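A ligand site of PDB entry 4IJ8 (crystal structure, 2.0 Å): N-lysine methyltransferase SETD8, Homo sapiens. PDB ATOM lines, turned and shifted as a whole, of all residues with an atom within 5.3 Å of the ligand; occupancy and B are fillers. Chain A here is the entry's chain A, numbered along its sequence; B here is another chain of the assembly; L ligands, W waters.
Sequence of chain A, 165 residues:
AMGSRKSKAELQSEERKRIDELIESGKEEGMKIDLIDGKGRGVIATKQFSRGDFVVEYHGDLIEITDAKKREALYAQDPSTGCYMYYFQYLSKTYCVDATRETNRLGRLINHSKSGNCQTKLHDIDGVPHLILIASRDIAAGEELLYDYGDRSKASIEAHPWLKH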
ATOM      1  N   GLY A  38      26.848 -16.702  -3.055  1.00  0.00           N
ATOM      2  CA  GLY A  38      25.529 -16.137  -3.465  1.00  0.00           C
ATOM      3  C   GLY A  38      24.561 -17.187  -4.010  1.00  0.00           C
ATOM      4  O   GLY A  38      23.365 -16.918  -4.156  1.00  0.00           O
ATOM      5  N   LYS A  39      25.031 -18.395  -4.235  1.00  0.00           N
ATOM      6  CA  LYS A  39      24.169 -19.445  -4.815  1.00  0.00           C
ATOM      7  C   LYS A  39      24.131 -20.722  -4.038  1.00  0.00           C
ATOM      8  O   LYS A  39      23.215 -21.502  -4.214  1.00  0.00           O
ATOM      9  CB  LYS A  39      24.626 -19.781  -6.221  1.00  0.00           C
ATOM     10  CG  LYS A  39      24.517 -18.635  -7.187  1.00  0.00           C
ATOM     11  CD  LYS A  39      25.141 -18.983  -8.516  1.00  0.00           C
ATOM     12  CE  LYS A  39      24.842 -17.917  -9.515  1.00  0.00           C
ATOM     13  NZ  LYS A  39      25.690 -18.119 -10.690  1.00  0.00           N
ATOM     14  N   GLY A  40      25.141 -21.001  -3.217  1.00  0.00           N
ATOM     15  CA  GLY A  40      25.217 -22.289  -2.547  1.00  0.00           C
ATOM     16  C   GLY A  40      26.043 -23.253  -3.368  1.00  0.00           C
ATOM     17  O   GLY A  40      27.118 -22.926  -3.801  1.00  0.00           O
ATOM     18  N   ARG A  41      25.525 -24.448  -3.592  1.00  0.00           N
ATOM     19  CA  ARG A  41      26.181 -25.396  -4.440  1.00  0.00           C
ATOM     20  C   ARG A  41      25.844 -25.049  -5.877  1.00  0.00           C
ATOM     21  O   ARG A  41      24.757 -24.563  -6.154  1.00  0.00           O
ATOM     22  CB  ARG A  41      25.706 -26.799  -4.128  1.00  0.00           C
ATOM     23  CG  ARG A  41      25.978 -27.248  -2.695  1.00  0.00           C
ATOM     24  CD  ARG A  41      25.307 -28.567  -2.381  1.00  0.00           C
ATOM     25  NE  ARG A  41      23.845 -28.424  -2.369  1.00  0.00           N
ATOM     26  CZ  ARG A  41      22.985 -29.410  -2.095  1.00  0.00           C
ATOM     27  NH1 ARG A  41      23.420 -30.647  -1.851  1.00  0.00           N
ATOM     28  NH2 ARG A  41      21.693 -29.165  -2.114  1.00  0.00           N
ATOM     29  N   GLY A  42      26.779 -25.278  -6.784  1.00  0.00           N
ATOM     30  CA  GLY A  42      26.484 -25.208  -8.216  1.00  0.00           C
ATOM     31  C   GLY A  42      27.324 -26.225  -8.945  1.00  0.00           C
ATOM     32  O   GLY A  42      28.150 -26.899  -8.354  1.00  0.00           O
ATOM     33  N   CYS A  83      12.017 -24.287  -6.955  1.00  0.00           N
ATOM     34  CA  CYS A  83      13.324 -24.372  -7.600  1.00  0.00           C
ATOM     35  C   CYS A  83      13.787 -25.825  -7.812  1.00  0.00           C
ATOM     36  O   CYS A  83      14.670 -26.085  -8.639  1.00  0.00           O
ATOM     37  CB  CYS A  83      14.413 -23.614  -6.822  1.00  0.00           C
ATOM     38  SG  CYS A  83      14.043 -21.900  -6.465  1.00  0.00           S
ATOM     39  N   TYR A  84      13.208 -26.755  -7.060  1.00  0.00           N
ATOM     40  CA  TYR A  84      13.594 -28.138  -7.095  1.00  0.00           C
ATOM     41  C   TYR A  84      12.535 -29.027  -7.717  1.00  0.00           C
ATOM     42  O   TYR A  84      12.585 -30.235  -7.556  1.00  0.00           O
ATOM     43  CB  TYR A  84      13.912 -28.639  -5.679  1.00  0.00           C
ATOM     44  CG  TYR A  84      15.098 -27.989  -5.027  1.00  0.00           C
ATOM     45  CD1 TYR A  84      14.982 -26.783  -4.332  1.00  0.00           C
ATOM     46  CD2 TYR A  84      16.374 -28.588  -5.086  1.00  0.00           C
ATOM     47  CE1 TYR A  84      16.092 -26.180  -3.710  1.00  0.00           C
ATOM     48  CE2 TYR A  84      17.465 -28.018  -4.461  1.00  0.00           C
ATOM     49  CZ  TYR A  84      17.315 -26.796  -3.784  1.00  0.00           C
ATOM     50  OH  TYR A  84      18.429 -26.237  -3.175  1.00  0.00           O
ATOM     51  N   GLU A 102      17.598 -35.069  -1.737  1.00  0.00           N
ATOM     52  CA  GLU A 102      19.028 -35.089  -1.979  1.00  0.00           C
ATOM     53  C   GLU A 102      19.399 -36.472  -2.556  1.00  0.00           C
ATOM     54  O   GLU A 102      18.988 -37.460  -2.027  1.00  0.00           O
ATOM     55  CB  GLU A 102      19.782 -34.864  -0.686  1.00  0.00           C
ATOM     56  CG  GLU A 102      19.742 -33.429  -0.220  1.00  0.00           C
ATOM     57  CD  GLU A 102      20.373 -32.481  -1.208  1.00  0.00           C
ATOM     58  OE1 GLU A 102      21.524 -32.739  -1.560  1.00  0.00           O
ATOM     59  OE2 GLU A 102      19.724 -31.492  -1.645  1.00  0.00           O
ATOM     60  N   ARG A 108      19.882 -31.453 -10.652  1.00  0.00           N
ATOM     61  CA  ARG A 108      19.180 -30.724  -9.597  1.00  0.00           C
ATOM     62  C   ARG A 108      20.055 -29.695  -8.858  1.00  0.00           C
ATOM     63  O   ARG A 108      19.511 -28.912  -8.051  1.00  0.00           O
ATOM     64  CB  ARG A 108      18.624 -31.689  -8.587  1.00  0.00           C
ATOM     65  CG  ARG A 108      19.642 -32.564  -7.859  1.00  0.00           C
ATOM     66  CD  ARG A 108      18.954 -33.541  -6.917  1.00  0.00           C
ATOM     67  NE  ARG A 108      18.128 -32.862  -5.919  1.00  0.00           N
ATOM     68  CZ  ARG A 108      18.589 -32.408  -4.755  1.00  0.00           C
ATOM     69  NH1 ARG A 108      19.873 -32.561  -4.451  1.00  0.00           N
ATOM     70  NH2 ARG A 108      17.780 -31.811  -3.914  1.00  0.00           N
ATOM     71  N   LEU A 109      21.383 -29.693  -9.100  1.00  0.00           N
ATOM     72  CA  LEU A 109      22.256 -28.733  -8.407  1.00  0.00           C
ATOM     73  C   LEU A 109      22.661 -27.586  -9.269  1.00  0.00           C
ATOM     74  O   LEU A 109      23.479 -26.762  -8.863  1.00  0.00           O
ATOM     75  CB  LEU A 109      23.492 -29.427  -7.851  1.00  0.00           C
ATOM     76  CG  LEU A 109      23.247 -30.476  -6.766  1.00  0.00           C
ATOM     77  CD1 LEU A 109      24.559 -31.151  -6.307  1.00  0.00           C
ATOM     78  CD2 LEU A 109      22.476 -29.923  -5.576  1.00  0.00           C
ATOM     79  N   ILE A 110      22.136 -27.552 -10.487  1.00  0.00           N
ATOM     80  CA  ILE A 110      22.450 -26.510 -11.449  1.00  0.00           C
ATOM     81  C   ILE A 110      21.598 -25.284 -11.143  1.00  0.00           C
ATOM     82  O   ILE A 110      20.383 -25.385 -10.964  1.00  0.00           O
ATOM     83  CB  ILE A 110      22.253 -27.009 -12.897  1.00  0.00           C
ATOM     84  CG1 ILE A 110      23.289 -28.116 -13.194  1.00  0.00           C
ATOM     85  CG2 ILE A 110      22.376 -25.846 -13.877  1.00  0.00           C
ATOM     86  CD1 ILE A 110      23.126 -28.807 -14.581  1.00  0.00           C
ATOM     87  N   ASN A 111      22.265 -24.116 -11.120  1.00  0.00           N
ATOM     88  CA  ASN A 111      21.650 -22.856 -10.760  1.00  0.00           C
ATOM     89  C   ASN A 111      20.991 -22.173 -11.959  1.00  0.00           C
ATOM     90  O   ASN A 111      21.062 -22.661 -13.109  1.00  0.00           O
ATOM     91  CB  ASN A 111      22.690 -21.969 -10.040  1.00  0.00           C
ATOM     92  CG  ASN A 111      23.032 -22.496  -8.654  1.00  0.00           C
ATOM     93  OD1 ASN A 111      22.142 -22.884  -7.873  1.00  0.00           O
ATOM     94  ND2 ASN A 111      24.294 -22.578  -8.363  1.00  0.00           N
ATOM     95  N   HIS A 112      20.307 -21.076 -11.671  1.00  0.00           N
ATOM     96  CA  HIS A 112      19.483 -20.364 -12.644  1.00  0.00           C
ATOM     97  C   HIS A 112      20.152 -19.191 -13.290  1.00  0.00           C
ATOM     98  O   HIS A 112      20.854 -18.403 -12.624  1.00  0.00           O
ATOM     99  CB  HIS A 112      18.209 -19.860 -11.967  1.00  0.00           C
ATOM    100  CG  HIS A 112      17.471 -18.809 -12.747  1.00  0.00           C
ATOM    101  ND1 HIS A 112      16.537 -19.118 -13.708  1.00  0.00           N
ATOM    102  CD2 HIS A 112      17.539 -17.457 -12.720  1.00  0.00           C
ATOM    103  CE1 HIS A 112      16.060 -18.014 -14.244  1.00  0.00           C
ATOM    104  NE2 HIS A 112      16.650 -16.987 -13.661  1.00  0.00           N
ATOM    105  N   SER A 113      19.889 -19.042 -14.588  1.00  0.00           N
ATOM    106  CA  SER A 113      20.088 -17.803 -15.289  1.00  0.00           C
ATOM    107  C   SER A 113      19.134 -17.766 -16.499  1.00  0.00           C
ATOM    108  O   SER A 113      18.919 -18.782 -17.150  1.00  0.00           O
ATOM    109  CB  SER A 113      21.521 -17.691 -15.809  1.00  0.00           C
ATOM    110  OG  SER A 113      21.680 -16.482 -16.470  1.00  0.00           O
ATOM    111  N   TYR A 149      15.130 -21.378 -15.094  1.00  0.00           N
ATOM    112  CA  TYR A 149      14.205 -22.152 -14.279  1.00  0.00           C
ATOM    113  C   TYR A 149      12.767 -22.032 -14.812  1.00  0.00           C
ATOM    114  O   TYR A 149      11.921 -22.825 -14.431  1.00  0.00           O
ATOM    115  CB  TYR A 149      14.282 -21.693 -12.814  1.00  0.00           C
ATOM    116  CG  TYR A 149      15.474 -22.255 -11.999  1.00  0.00           C
ATOM    117  CD1 TYR A 149      16.553 -22.917 -12.607  1.00  0.00           C
ATOM    118  CD2 TYR A 149      15.509 -22.086 -10.620  1.00  0.00           C
ATOM    119  CE1 TYR A 149      17.598 -23.446 -11.849  1.00  0.00           C
ATOM    120  CE2 TYR A 149      16.541 -22.576  -9.858  1.00  0.00           C
ATOM    121  CZ  TYR A 149      17.576 -23.250 -10.472  1.00  0.00           C
ATOM    122  OH  TYR A 149      18.611 -23.725  -9.709  1.00  0.00           O
ATOM    123  N   HIS A 160      12.705 -14.807  -4.504  1.00  0.00           N
ATOM    124  CA  HIS A 160      13.893 -15.186  -5.265  1.00  0.00           C
ATOM    125  C   HIS A 160      14.131 -14.194  -6.447  1.00  0.00           C
ATOM    126  O   HIS A 160      13.964 -14.543  -7.622  1.00  0.00           O
ATOM    127  CB  HIS A 160      13.723 -16.599  -5.836  1.00  0.00           C
ATOM    128  CG  HIS A 160      13.375 -17.644  -4.833  1.00  0.00           C
ATOM    129  ND1 HIS A 160      14.242 -18.020  -3.817  1.00  0.00           N
ATOM    130  CD2 HIS A 160      12.273 -18.425  -4.702  1.00  0.00           C
ATOM    131  CE1 HIS A 160      13.673 -18.973  -3.083  1.00  0.00           C
ATOM    132  NE2 HIS A 160      12.474 -19.230  -3.599  1.00  0.00           N
ATOM    133  N   TRP A 162      16.629 -13.011  -7.919  1.00  0.00           N
ATOM    134  CA  TRP A 162      17.632 -13.455  -8.866  1.00  0.00           C
ATOM    135  C   TRP A 162      16.979 -14.171 -10.055  1.00  0.00           C
ATOM    136  O   TRP A 162      17.632 -14.347 -11.089  1.00  0.00           O
ATOM    137  CB  TRP A 162      18.666 -14.351  -8.214  1.00  0.00           C
ATOM    138  CG  TRP A 162      18.115 -15.396  -7.321  1.00  0.00           C
ATOM    139  CD1 TRP A 162      18.019 -15.344  -5.950  1.00  0.00           C
ATOM    140  CD2 TRP A 162      17.566 -16.661  -7.715  1.00  0.00           C
ATOM    141  NE1 TRP A 162      17.471 -16.488  -5.476  1.00  0.00           N
ATOM    142  CE2 TRP A 162      17.167 -17.315  -6.520  1.00  0.00           C
ATOM    143  CE3 TRP A 162      17.350 -17.307  -8.955  1.00  0.00           C
ATOM    144  CZ2 TRP A 162      16.555 -18.597  -6.527  1.00  0.00           C
ATOM    145  CZ3 TRP A 162      16.751 -18.584  -8.966  1.00  0.00           C
ATOM    146  CH2 TRP A 162      16.367 -19.213  -7.767  1.00  0.00           C
ATOM    147  N   PRO B  79      17.558 -29.576   2.469  1.00  0.00           N
ATOM    148  CA  PRO B  79      18.017 -28.389   1.711  1.00  0.00           C
ATOM    149  C   PRO B  79      16.917 -27.680   0.915  1.00  0.00           C
ATOM    150  O   PRO B  79      16.820 -26.458   0.931  1.00  0.00           O
ATOM    151  CB  PRO B  79      19.113 -28.969   0.776  1.00  0.00           C
ATOM    152  CG  PRO B  79      19.546 -30.217   1.461  1.00  0.00           C
ATOM    153  CD  PRO B  79      18.305 -30.783   2.096  1.00  0.00           C
ATOM    154  N   GLU B 158      25.613 -26.195   3.021  1.00  0.00           N
ATOM    155  CA  GLU B 158      26.290 -25.893   1.767  1.00  0.00           C
ATOM    156  C   GLU B 158      25.365 -25.118   0.822  1.00  0.00           C
ATOM    157  O   GLU B 158      25.774 -24.151   0.175  1.00  0.00           O
ATOM    158  CB  GLU B 158      26.771 -27.157   1.125  1.00  0.00           C
ATOM    159  CG  GLU B 158      27.849 -27.869   1.922  1.00  0.00           C
ATOM    160  CD  GLU B 158      28.413 -29.066   1.195  1.00  0.00           C
ATOM    161  OE1 GLU B 158      29.578 -29.354   1.399  1.00  0.00           O
ATOM    162  OE2 GLU B 158      27.716 -29.710   0.404  1.00  0.00           O
ATOM    163  N   ALA B 159      24.104 -25.535   0.760  1.00  0.00           N
ATOM    164  CA  ALA B 159      23.078 -24.842  -0.044  1.00  0.00           C
ATOM    165  C   ALA B 159      22.769 -23.458   0.426  1.00  0.00           C
ATOM    166  O   ALA B 159      22.467 -22.569  -0.404  1.00  0.00           O
ATOM    167  CB  ALA B 159      21.800 -25.683  -0.089  1.00  0.00           C
ATOM    168  N   HIS B 160      22.801 -23.278   1.753  1.00  0.00           N
ATOM    169  CA  HIS B 160      22.319 -22.080   2.416  1.00  0.00           C
ATOM    170  C   HIS B 160      23.318 -21.591   3.514  1.00  0.00           C
ATOM    171  O   HIS B 160      23.047 -21.686   4.709  1.00  0.00           O
ATOM    172  CB  HIS B 160      20.948 -22.353   3.109  1.00  0.00           C
ATOM    173  CG  HIS B 160      19.907 -22.954   2.213  1.00  0.00           C
ATOM    174  ND1 HIS B 160      19.336 -22.276   1.150  1.00  0.00           N
ATOM    175  CD2 HIS B 160      19.284 -24.158   2.268  1.00  0.00           C
ATOM    176  CE1 HIS B 160      18.451 -23.060   0.563  1.00  0.00           C
ATOM    177  NE2 HIS B 160      18.393 -24.203   1.223  1.00  0.00           N
HETATM  178  N1  LIG L   1      22.211 -23.957  -5.123  1.00  0.00           N
HETATM  179  C1  LIG L   1      21.353 -25.129  -5.002  1.00  0.00           C
HETATM  180  C2  LIG L   1      21.804 -25.969  -3.834  1.00  0.00           C
HETATM  181  O1  LIG L   1      22.904 -25.717  -3.237  1.00  0.00           O
HETATM  182  O2  LIG L   1      21.052 -26.876  -3.463  1.00  0.00           O
HETATM  183  C3  LIG L   1      21.335 -25.945  -6.288  1.00  0.00           C
HETATM  184  C4  LIG L   1      20.223 -25.476  -7.271  1.00  0.00           C
HETATM  185  S1  LIG L   1      18.643 -25.557  -6.624  1.00  0.00           S
HETATM  186  C5  LIG L   1      17.708 -26.383  -7.770  1.00  0.00           C
HETATM  187  C6  LIG L   1      17.825 -24.060  -6.367  1.00  0.00           C
HETATM  188  C7  LIG L   1      18.380 -23.068  -5.323  1.00  0.00           C
HETATM  189  O3  LIG L   1      19.667 -22.568  -5.769  1.00  0.00           O
HETATM  190  C8  LIG L   1      17.577 -21.785  -5.180  1.00  0.00           C
HETATM  191  O4  LIG L   1      16.348 -21.861  -4.416  1.00  0.00           O
HETATM  192  C9  LIG L   1      18.602 -20.796  -4.656  1.00  0.00           C
HETATM  193  O5  LIG L   1      18.911 -20.919  -3.242  1.00  0.00           O
HETATM  194  C10 LIG L   1      19.827 -21.195  -5.450  1.00  0.00           C
HETATM  195  N2  LIG L   1      19.997 -20.466  -6.718  1.00  0.00           N
HETATM  196  C11 LIG L   1      19.811 -20.980  -7.957  1.00  0.00           C
HETATM  197  N3  LIG L   1      20.107 -20.087  -8.902  1.00  0.00           N
HETATM  198  C12 LIG L   1      20.495 -18.964  -8.245  1.00  0.00           C
HETATM  199  C13 LIG L   1      20.892 -17.662  -8.661  1.00  0.00           C
HETATM  200  N4  LIG L   1      20.976 -17.324  -9.976  1.00  0.00           N
HETATM  201  N5  LIG L   1      21.212 -16.775  -7.700  1.00  0.00           N
HETATM  202  C14 LIG L   1      21.144 -17.057  -6.395  1.00  0.00           C
HETATM  203  N6  LIG L   1      20.741 -18.259  -5.952  1.00  0.00           N
HETATM  204  C15 LIG L   1      20.433 -19.232  -6.843  1.00  0.00           C
HETATM  205  O   HOH W   1      20.394 -14.419 -11.300  1.00  0.00           O
HETATM  206  O   HOH W   2      20.787 -22.914  -2.685  1.00  0.00           O
HETATM  207  O   HOH W   3      22.411 -14.356  -7.825  1.00  0.00           O
HETATM  208  O   HOH W   4      17.507 -19.398  -1.343  1.00  0.00           O
HETATM  209  O   HOH W   5      20.654 -18.569  -3.055  1.00  0.00           O
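The side-chain hydroxyl (OH) of Tyr 84 lies within hydrogen-bond range of an oxygen (O2) of the ligand (2.7 Å).
The backbone NH of Arg 41 lies within hydrogen-bond range of an oxygen (O1) of the ligand (2.9 Å).
O of Arg 41 is in hydrogen-bond range of N1 of the ligand, at 2.8 Å.
The guanidinium group (NH2) of Arg 41 is in salt-bridge range of an oxygen (O2) of the ligand (2.7 Å).
O of Lys 39 sits at hydrogen-bond distance from N1 of the ligand.
The backbone NH (N) of His 112 sits at hydrogen-bond distance from a nitrogen (N3) of the ligand, at 2.9 Å.
A nitrogen (N4) of the ligand sits at hydrogen-bond distance from the backbone carbonyl oxygen (O) of His 112.
N1 of the ligand is in hydrogen-bond range of OD1 of Asn 111 (3.0 Å).
O4 of the ligand is in hydrogen-bond range of SG of Cys 83 (3.1 Å).
ND2 of Asn 111 sits at hydrogen-bond distance from O of Arg 41 (3.0 Å).
The guanidinium group (NH1) of Arg 41 lies within salt-bridge range of the side-chain carboxylate (OE1) of Glu 102 (2.8 Å).
ND1 of His 112 sits at hydrogen-bond distance from N of Tyr 149 (3.0 Å).
The guanidinium group (NH2) of Arg 108 lies within salt-bridge range of the side-chain carboxylate (OE2) of Glu 102.
OH of Tyr 149 lies within hydrogen-bond range of O of Ile 110 (2.7 Å).
The backbone carbonyl oxygen (O) of Gly 38 lies close to a nitrogen (N6) of the ligand, 3.5 Å away.
S1 of the ligand sits close to O of Arg 108 (3.7 Å).
OH of Tyr 149 lies close to S1 of the ligand (3.6 Å).
Gly 40 touches the ligand (C to O1, 3.99 Å).
O of Leu 109 touches C3 of the ligand, 3.4 Å away.
Ile 110 touches the ligand.
CG of Trp 162 touches N5 of the ligand (3.4 Å).
Ala 159 of chain B touches the ligand.
Hydrophobic or aromatic side chains within 4 Å of the ligand: Tyr 84, Leu 109, His 112, Trp 162 and Ala 159 of chain B.
Water W2 lies within hydrogen-bond range of O5 of the ligand, O of Ala 159 of chain B and O of Lys 39.
Water W5 lies within hydrogen-bond range of N6 of the ligand (2.9 Å) and O of Gly 38 (3.4 Å).
Water W1 bridges the backbone carbonyl oxygen (O) of Trp 162 (2.8 Å) and a nitrogen (N4) of the ligand (3.2 Å).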
